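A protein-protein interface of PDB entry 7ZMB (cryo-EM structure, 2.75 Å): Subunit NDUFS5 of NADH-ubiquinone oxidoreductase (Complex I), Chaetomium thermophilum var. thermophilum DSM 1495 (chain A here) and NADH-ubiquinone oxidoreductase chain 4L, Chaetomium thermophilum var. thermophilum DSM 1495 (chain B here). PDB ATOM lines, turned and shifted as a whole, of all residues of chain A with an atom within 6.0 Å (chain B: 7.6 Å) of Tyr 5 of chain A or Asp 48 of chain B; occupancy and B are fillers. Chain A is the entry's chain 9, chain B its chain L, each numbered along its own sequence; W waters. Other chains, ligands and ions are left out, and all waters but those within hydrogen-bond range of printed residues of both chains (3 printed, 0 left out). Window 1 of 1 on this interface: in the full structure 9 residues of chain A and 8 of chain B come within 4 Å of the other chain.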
ATOM      1  N   MET A   1     -19.486  -2.015  -7.388  1.00  0.00           N
ATOM      2  CA  MET A   1     -19.159  -0.565  -7.267  1.00  0.00           C
ATOM      3  C   MET A   1     -19.237  -0.119  -5.810  1.00  0.00           C
ATOM      4  O   MET A   1     -19.283  -0.998  -4.947  1.00  0.00           O
ATOM      5  CB  MET A   1     -20.037   0.313  -8.157  1.00  0.00           C
ATOM      6  N   SER A   3     -21.552   1.250  -3.891  1.00  0.00           N
ATOM      7  CA  SER A   3     -22.814   1.112  -3.115  1.00  0.00           C
ATOM      8  C   SER A   3     -22.913  -0.123  -2.203  1.00  0.00           C
ATOM      9  O   SER A   3     -23.339   0.064  -1.068  1.00  0.00           O
ATOM     10  CB  SER A   3     -23.991   1.183  -4.048  1.00  0.00           C
ATOM     11  OG  SER A   3     -24.082   0.015  -4.849  1.00  0.00           O
ATOM     12  N   GLY A   4     -22.625  -1.336  -2.670  1.00  0.00           N
ATOM     13  CA  GLY A   4     -22.809  -2.515  -1.806  1.00  0.00           C
ATOM     14  C   GLY A   4     -23.963  -3.357  -2.291  1.00  0.00           C
ATOM     15  O   GLY A   4     -24.252  -4.381  -1.666  1.00  0.00           O
ATOM     16  N   TYR A   5     -24.589  -2.935  -3.385  1.00  0.00           N
ATOM     17  CA  TYR A   5     -25.796  -3.631  -3.889  1.00  0.00           C
ATOM     18  C   TYR A   5     -25.553  -3.958  -5.355  1.00  0.00           C
ATOM     19  O   TYR A   5     -25.480  -3.037  -6.176  1.00  0.00           O
ATOM     20  CB  TYR A   5     -27.015  -2.744  -3.640  1.00  0.00           C
ATOM     21  CG  TYR A   5     -27.188  -2.354  -2.195  1.00  0.00           C
ATOM     22  CD1 TYR A   5     -27.835  -3.193  -1.306  1.00  0.00           C
ATOM     23  CD2 TYR A   5     -26.669  -1.167  -1.707  1.00  0.00           C
ATOM     24  CE1 TYR A   5     -27.977  -2.857   0.029  1.00  0.00           C
ATOM     25  CE2 TYR A   5     -26.794  -0.821  -0.373  1.00  0.00           C
ATOM     26  CZ  TYR A   5     -27.456  -1.665   0.498  1.00  0.00           C
ATOM     27  OH  TYR A   5     -27.593  -1.328   1.812  1.00  0.00           O
ATOM     28  N   GLY A   6     -25.426  -5.243  -5.662  1.00  0.00           N
ATOM     29  CA  GLY A   6     -25.133  -5.658  -7.037  1.00  0.00           C
ATOM     30  C   GLY A   6     -26.368  -6.046  -7.811  1.00  0.00           C
ATOM     31  O   GLY A   6     -27.475  -5.905  -7.271  1.00  0.00           O
ATOM     32  N   LEU A   7     -26.180  -6.654  -8.984  1.00  0.00           N
ATOM     33  CA  LEU A   7     -27.300  -6.962  -9.909  1.00  0.00           C
ATOM     34  C   LEU A   7     -28.173  -8.156  -9.491  1.00  0.00           C
ATOM     35  O   LEU A   7     -29.370  -8.122  -9.828  1.00  0.00           O
ATOM     36  CB  LEU A   7     -26.732  -7.099 -11.323  1.00  0.00           C
ATOM     37  CG  LEU A   7     -25.961  -5.881 -11.822  1.00  0.00           C
ATOM     38  CD1 LEU A   7     -25.230  -6.184 -13.116  1.00  0.00           C
ATOM     39  CD2 LEU A   7     -26.883  -4.687 -11.993  1.00  0.00           C
ATOM     40  N   ASN A   8     -27.639  -9.138  -8.766  1.00  0.00           N
ATOM     41  CA  ASN A   8     -28.434 -10.347  -8.400  1.00  0.00           C
ATOM     42  C   ASN A   8     -29.100 -10.220  -7.029  1.00  0.00           C
ATOM     43  O   ASN A   8     -29.668 -11.215  -6.575  1.00  0.00           O
ATOM     44  CB  ASN A   8     -27.661 -11.654  -8.599  1.00  0.00           C
ATOM     45  CG  ASN A   8     -26.584 -11.949  -7.572  1.00  0.00           C
ATOM     46  OD1 ASN A   8     -26.851 -12.060  -6.380  1.00  0.00           O
ATOM     47  ND2 ASN A   8     -25.360 -12.139  -8.033  1.00  0.00           N
ATOM     48  N   GLY A  10     -27.347  -9.657  -4.522  1.00  0.00           N
ATOM     49  CA  GLY A  10     -26.178  -9.840  -3.654  1.00  0.00           C
ATOM     50  C   GLY A  10     -25.315  -8.593  -3.669  1.00  0.00           C
ATOM     51  O   GLY A  10     -25.722  -7.589  -4.249  1.00  0.00           O
ATOM     52  N   PRO A  11     -24.120  -8.576  -3.028  1.00  0.00           N
ATOM     53  CA  PRO A  11     -23.309  -7.351  -2.923  1.00  0.00           C
ATOM     54  C   PRO A  11     -22.444  -7.003  -4.143  1.00  0.00           C
ATOM     55  O   PRO A  11     -22.087  -7.886  -4.874  1.00  0.00           O
ATOM     56  CB  PRO A  11     -22.401  -7.620  -1.725  1.00  0.00           C
ATOM     57  CG  PRO A  11     -22.881  -8.910  -1.117  1.00  0.00           C
ATOM     58  CD  PRO A  11     -23.465  -9.667  -2.280  1.00  0.00           C
ATOM     59  N   SER A  12     -22.154  -5.724  -4.350  1.00  0.00           N
ATOM     60  CA  SER A  12     -21.372  -5.282  -5.534  1.00  0.00           C
ATOM     61  C   SER A  12     -19.940  -5.855  -5.509  1.00  0.00           C
ATOM     62  O   SER A  12     -19.341  -5.861  -4.436  1.00  0.00           O
ATOM     63  CB  SER A  12     -21.436  -3.779  -5.665  1.00  0.00           C
ATOM     64  OG  SER A  12     -20.874  -3.136  -4.539  1.00  0.00           O
ATOM     65  N   ARG A  13     -19.413  -6.308  -6.649  1.00  0.00           N
ATOM     66  CA  ARG A  13     -18.082  -6.982  -6.672  1.00  0.00           C
ATOM     67  C   ARG A  13     -16.925  -6.058  -6.276  1.00  0.00           C
ATOM     68  O   ARG A  13     -15.900  -6.593  -5.863  1.00  0.00           O
ATOM     69  CB  ARG A  13     -17.791  -7.525  -8.076  1.00  0.00           C
ATOM     70  CG  ARG A  13     -17.916  -6.505  -9.191  1.00  0.00           C
ATOM     71  CD  ARG A  13     -17.503  -7.090 -10.525  1.00  0.00           C
ATOM     72  NE  ARG A  13     -17.279  -6.002 -11.459  1.00  0.00           N
ATOM     73  CZ  ARG A  13     -16.108  -5.412 -11.629  1.00  0.00           C
ATOM     74  NH1 ARG A  13     -15.984  -4.417 -12.487  1.00  0.00           N
ATOM     75  NH2 ARG A  13     -15.065  -5.826 -10.938  1.00  0.00           N
ATOM     76  N   CYS A  14     -17.080  -4.744  -6.396  1.00  0.00           N
ATOM     77  CA  CYS A  14     -16.027  -3.812  -6.007  1.00  0.00           C
ATOM     78  C   CYS A  14     -16.271  -3.194  -4.643  1.00  0.00           C
ATOM     79  O   CYS A  14     -15.551  -2.273  -4.256  1.00  0.00           O
ATOM     80  CB  CYS A  14     -15.864  -2.707  -7.054  1.00  0.00           C
ATOM     81  SG  CYS A  14     -15.072  -3.230  -8.577  1.00  0.00           S
ATOM     82  N   PHE A  15     -17.270  -3.674  -3.912  1.00  0.00           N
ATOM     83  CA  PHE A  15     -17.520  -3.149  -2.576  1.00  0.00           C
ATOM     84  C   PHE A  15     -16.398  -3.430  -1.581  1.00  0.00           C
ATOM     85  O   PHE A  15     -16.071  -2.519  -0.803  1.00  0.00           O
ATOM     86  CB  PHE A  15     -18.863  -3.666  -2.059  1.00  0.00           C
ATOM     87  CG  PHE A  15     -19.369  -2.907  -0.882  1.00  0.00           C
ATOM     88  CD1 PHE A  15     -19.543  -1.539  -0.961  1.00  0.00           C
ATOM     89  CD2 PHE A  15     -19.647  -3.547   0.306  1.00  0.00           C
ATOM     90  CE1 PHE A  15     -19.990  -0.835   0.117  1.00  0.00           C
ATOM     91  CE2 PHE A  15     -20.099  -2.840   1.387  1.00  0.00           C
ATOM     92  CZ  PHE A  15     -20.277  -1.486   1.294  1.00  0.00           C
ATOM     93  N   LEU B  42     -24.904   1.285 -19.051  1.00  0.00           N
ATOM     94  CA  LEU B  42     -23.821   0.428 -19.516  1.00  0.00           C
ATOM     95  C   LEU B  42     -22.692   0.328 -18.498  1.00  0.00           C
ATOM     96  O   LEU B  42     -22.137  -0.753 -18.294  1.00  0.00           O
ATOM     97  CB  LEU B  42     -23.309   0.936 -20.858  1.00  0.00           C
ATOM     98  CG  LEU B  42     -24.197   0.427 -21.987  1.00  0.00           C
ATOM     99  CD1 LEU B  42     -23.939   1.163 -23.279  1.00  0.00           C
ATOM    100  CD2 LEU B  42     -23.947  -1.038 -22.156  1.00  0.00           C
ATOM    101  N   SER B  43     -22.329   1.434 -17.855  1.00  0.00           N
ATOM    102  CA  SER B  43     -21.343   1.448 -16.737  1.00  0.00           C
ATOM    103  C   SER B  43     -21.797   0.586 -15.560  1.00  0.00           C
ATOM    104  O   SER B  43     -20.987  -0.187 -15.053  1.00  0.00           O
ATOM    105  CB  SER B  43     -21.065   2.842 -16.312  1.00  0.00           C
ATOM    106  OG  SER B  43     -20.440   3.549 -17.370  1.00  0.00           O
ATOM    107  N   SER B  44     -23.037   0.732 -15.134  1.00  0.00           N
ATOM    108  CA  SER B  44     -23.566  -0.027 -13.981  1.00  0.00           C
ATOM    109  C   SER B  44     -23.469  -1.540 -14.207  1.00  0.00           C
ATOM    110  O   SER B  44     -23.296  -2.259 -13.208  1.00  0.00           O
ATOM    111  CB  SER B  44     -24.957   0.414 -13.732  1.00  0.00           C
ATOM    112  OG  SER B  44     -25.002   1.822 -13.779  1.00  0.00           O
ATOM    113  N   LEU B  45     -23.607  -2.021 -15.438  1.00  0.00           N
ATOM    114  CA  LEU B  45     -23.471  -3.473 -15.701  1.00  0.00           C
ATOM    115  C   LEU B  45     -22.010  -3.875 -15.558  1.00  0.00           C
ATOM    116  O   LEU B  45     -21.755  -4.936 -15.003  1.00  0.00           O
ATOM    117  CB  LEU B  45     -24.002  -3.715 -17.115  1.00  0.00           C
ATOM    118  CG  LEU B  45     -23.814  -5.115 -17.694  1.00  0.00           C
ATOM    119  CD1 LEU B  45     -24.594  -6.147 -16.896  1.00  0.00           C
ATOM    120  CD2 LEU B  45     -24.239  -5.142 -19.150  1.00  0.00           C
ATOM    121  N   ASN B  46     -21.097  -3.028 -15.991  1.00  0.00           N
ATOM    122  CA  ASN B  46     -19.632  -3.265 -15.860  1.00  0.00           C
ATOM    123  C   ASN B  46     -19.183  -3.259 -14.398  1.00  0.00           C
ATOM    124  O   ASN B  46     -18.220  -3.961 -14.093  1.00  0.00           O
ATOM    125  CB  ASN B  46     -18.864  -2.223 -16.670  1.00  0.00           C
ATOM    126  CG  ASN B  46     -19.143  -2.261 -18.156  1.00  0.00           C
ATOM    127  OD1 ASN B  46     -18.825  -1.315 -18.867  1.00  0.00           O
ATOM    128  ND2 ASN B  46     -19.734  -3.342 -18.634  1.00  0.00           N
ATOM    129  N   MET B  47     -19.803  -2.444 -13.541  1.00  0.00           N
ATOM    130  CA  MET B  47     -19.382  -2.316 -12.121  1.00  0.00           C
ATOM    131  C   MET B  47     -20.313  -3.068 -11.167  1.00  0.00           C
ATOM    132  O   MET B  47     -20.204  -2.803  -9.971  1.00  0.00           O
ATOM    133  CB  MET B  47     -19.300  -0.847 -11.712  1.00  0.00           C
ATOM    134  CG  MET B  47     -18.596   0.016 -12.738  1.00  0.00           C
ATOM    135  SD  MET B  47     -18.430   1.737 -12.225  1.00  0.00           S
ATOM    136  CE  MET B  47     -20.089   2.360 -12.485  1.00  0.00           C
ATOM    137  N   ASP B  48     -21.192  -3.948 -11.648  1.00  0.00           N
ATOM    138  CA  ASP B  48     -22.090  -4.761 -10.772  1.00  0.00           C
ATOM    139  C   ASP B  48     -22.891  -3.840  -9.843  1.00  0.00           C
ATOM    140  O   ASP B  48     -22.965  -4.145  -8.660  1.00  0.00           O
ATOM    141  CB  ASP B  48     -21.337  -5.919 -10.104  1.00  0.00           C
ATOM    142  CG  ASP B  48     -22.219  -6.906  -9.355  1.00  0.00           C
ATOM    143  OD1 ASP B  48     -21.806  -7.340  -8.263  1.00  0.00           O
ATOM    144  OD2 ASP B  48     -23.307  -7.236  -9.868  1.00  0.00           O
ATOM    145  N   ASP B  49     -23.413  -2.717 -10.335  1.00  0.00           N
ATOM    146  CA  ASP B  49     -24.082  -1.741  -9.441  1.00  0.00           C
ATOM    147  C   ASP B  49     -25.568  -1.648  -9.782  1.00  0.00           C
ATOM    148  O   ASP B  49     -25.897  -1.323 -10.929  1.00  0.00           O
ATOM    149  CB  ASP B  49     -23.420  -0.375  -9.575  1.00  0.00           C
ATOM    150  CG  ASP B  49     -23.707   0.538  -8.392  1.00  0.00           C
ATOM    151  OD1 ASP B  49     -24.367   0.081  -7.445  1.00  0.00           O
ATOM    152  OD2 ASP B  49     -23.267   1.696  -8.425  1.00  0.00           O
ATOM    153  N   ILE B  50     -26.433  -1.900  -8.808  1.00  0.00           N
ATOM    154  CA  ILE B  50     -27.886  -1.735  -9.064  1.00  0.00           C
ATOM    155  C   ILE B  50     -28.216  -0.240  -8.952  1.00  0.00           C
ATOM    156  O   ILE B  50     -29.292   0.159  -9.409  1.00  0.00           O
ATOM    157  CB  ILE B  50     -28.714  -2.675  -8.155  1.00  0.00           C
ATOM    158  CG1 ILE B  50     -30.053  -3.063  -8.782  1.00  0.00           C
ATOM    159  CG2 ILE B  50     -28.877  -2.105  -6.761  1.00  0.00           C
ATOM    160  CD1 ILE B  50     -29.942  -3.617 -10.178  1.00  0.00           C
ATOM    161  N   ILE B  51     -27.315   0.546  -8.364  1.00  0.00           N
ATOM    162  CA  ILE B  51     -27.574   1.999  -8.140  1.00  0.00           C
ATOM    163  C   ILE B  51     -27.658   2.715  -9.479  1.00  0.00           C
ATOM    164  O   ILE B  51     -28.492   3.613  -9.606  1.00  0.00           O
ATOM    165  CB  ILE B  51     -26.584   2.632  -7.136  1.00  0.00           C
ATOM    166  CG1 ILE B  51     -26.874   2.133  -5.722  1.00  0.00           C
ATOM    167  CG2 ILE B  51     -26.595   4.150  -7.197  1.00  0.00           C
ATOM    168  CD1 ILE B  51     -28.336   1.972  -5.450  1.00  0.00           C
ATOM    169  N   GLY B  52     -26.834   2.322 -10.436  1.00  0.00           N
ATOM    170  CA  GLY B  52     -26.899   2.923 -11.776  1.00  0.00           C
ATOM    171  C   GLY B  52     -28.211   2.676 -12.470  1.00  0.00           C
ATOM    172  O   GLY B  52     -28.675   3.588 -13.146  1.00  0.00           O
HETATM  173  O   HOH W   1     -24.487  -9.787  -9.540  1.00  0.00           O
HETATM  174  O   HOH W   2     -19.749  -6.579 -13.606  1.00  0.00           O
HETATM  175  O   HOH W   3     -22.442   3.565  -5.827  1.00  0.00           O
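Among the printed residues, pairs that only touch across the chains: Gly 6 of chain A with Asp 48 of chain B, Ser 12 of chain A with Asp 48 of chain B, Ser 3 of chain A with Ile 51 of chain B, Met 1 of chain A with Asp 49 of chain B, Tyr 5 of chain A with Asp 49 of chain B, Gly 6 of chain A with Ile 50 of chain B, Leu 7 of chain A with Asp 49 of chain B, Tyr 5 of chain A with Asp 48 of chain B, Leu 7 of chain A with Ile 50 of chain B and Leu 7 of chain A with Leu 45 of chain B.
Of the 13 printed residues of chain A, 8 touch a printed residue of chain B.
Along chain A the printed residues that touch a printed residue of chain B span positions 1 to 13.
Of the 11 printed residues of chain B, 7 touch a printed residue of chain A.
Hydrophobic or aromatic side chains of chain B within 4 Å of the printed part of chain A: Leu 45, Met 47, Ile 50 and Ile 51.
Among the printed residues, no Asp or Glu carboxylate lies within 4 Å of a Lys or Arg side-chain nitrogen of the other chain.
Water W1 lies within hydrogen-bond range of OD2 of Asp 48 of chain B and ND2 of Asn 8 of chain A.
Water W2 lies within hydrogen-bond range of the backbone carbonyl oxygen (O) of Leu 45 of chain B (2.9 Å), the backbone carbonyl oxygen (O) of Asn 46 of chain B (3.1 Å) and the guanidinium group (NE) of Arg 13 of chain A (3.3 Å).
Water W3 bridges N of Ser 3 of chain A and OD2 of Asp 49 of chain B.
The backbone carbonyl oxygen (O) of Leu 42 of chain B sits close to the side-chain amide oxygen (OD1) of Asn 46 of chain B (3.4 Å).
The backbone NH (N) of Ile 51 of chain B is in hydrogen-bond range of the side-chain carboxylate (OD1) of Asp 49 of chain B (3.1 Å).
The side-chain hydroxyl of Ser 12 of chain A is in hydrogen-bond range of the backbone carbonyl oxygen of Met 1 of chain A.
The side-chain hydroxyl (OG) of Ser 3 of chain A sits at hydrogen-bond distance from the backbone NH (N) of Tyr 5 of chain A, at 3.3 Å.
The side-chain hydroxyl (OG) of Ser 12 of chain A is in hydrogen-bond range of the backbone NH (N) of Gly 4 of chain A (3.1 Å).
NH2 of Arg 13 of chain A sits at hydrogen-bond distance from SG of Cys 14 of chain A.
Tyr 5 of chain A touches just these residues of chain B: Asp 48 (3.7 Å), Asp 49 (3.5 Å) and Ile 50 (3.0 Å).
Of chain A, only Tyr 5, Gly 6, Leu 7, Pro 11, Ser 12 and Arg 13 come within 4 Å of Asp 48 of chain B.
No residue of chain B comes within 4 Å of Gly 4 of chain A.
Of the printed residues of chain B, Met 1 of chain A touches Met 47 and Asp 49.
Of the printed residues of chain B, Ser 3 of chain A touches Asp 49 and Ile 51.
Of the printed residues of chain A, Asp 49 of chain B touches Met 1, Ser 3, Tyr 5 and Leu 7.
Of the printed residues of chain A, Ile 51 of chain B touches Ser 3.
Printed residues of chain B within 4 Å of Arg 13 of chain A: Asn 46 and Asp 48.
The nearest printed residue of chain A that does not touch Leu 45 of chain B is Arg 13 of chain A (5.8 Å).
The backbone carbonyl oxygen (O) of Asn 46 of chain B sits at hydrogen-bond distance from the guanidinium group (NH1) of Arg 13 of chain A, at 2.8 Å.
O of Met 47 of chain B is in hydrogen-bond range of N of Met 1 of chain A, 2.8 Å away.
OD2 of Asp 48 of chain B lies within hydrogen-bond range of N of Leu 7 of chain A, at 3.1 Å.
OD1 of Asp 48 of chain B is in hydrogen-bond range of N of Arg 13 of chain A, 3.1 Å away.
The side-chain carboxylate (OD1) of Asp 49 of chain B is in hydrogen-bond range of the side-chain hydroxyl (OG) of Ser 3 of chain A, 2.6 Å away.
The backbone carbonyl oxygen of Tyr 5 of chain A sits at hydrogen-bond distance from the backbone NH of Ile 50 of chain B, at 3.0 Å.
The side-chain carboxylate of Asp 48 of chain B lies close to the backbone carbonyl oxygen of Pro 11 of chain A.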
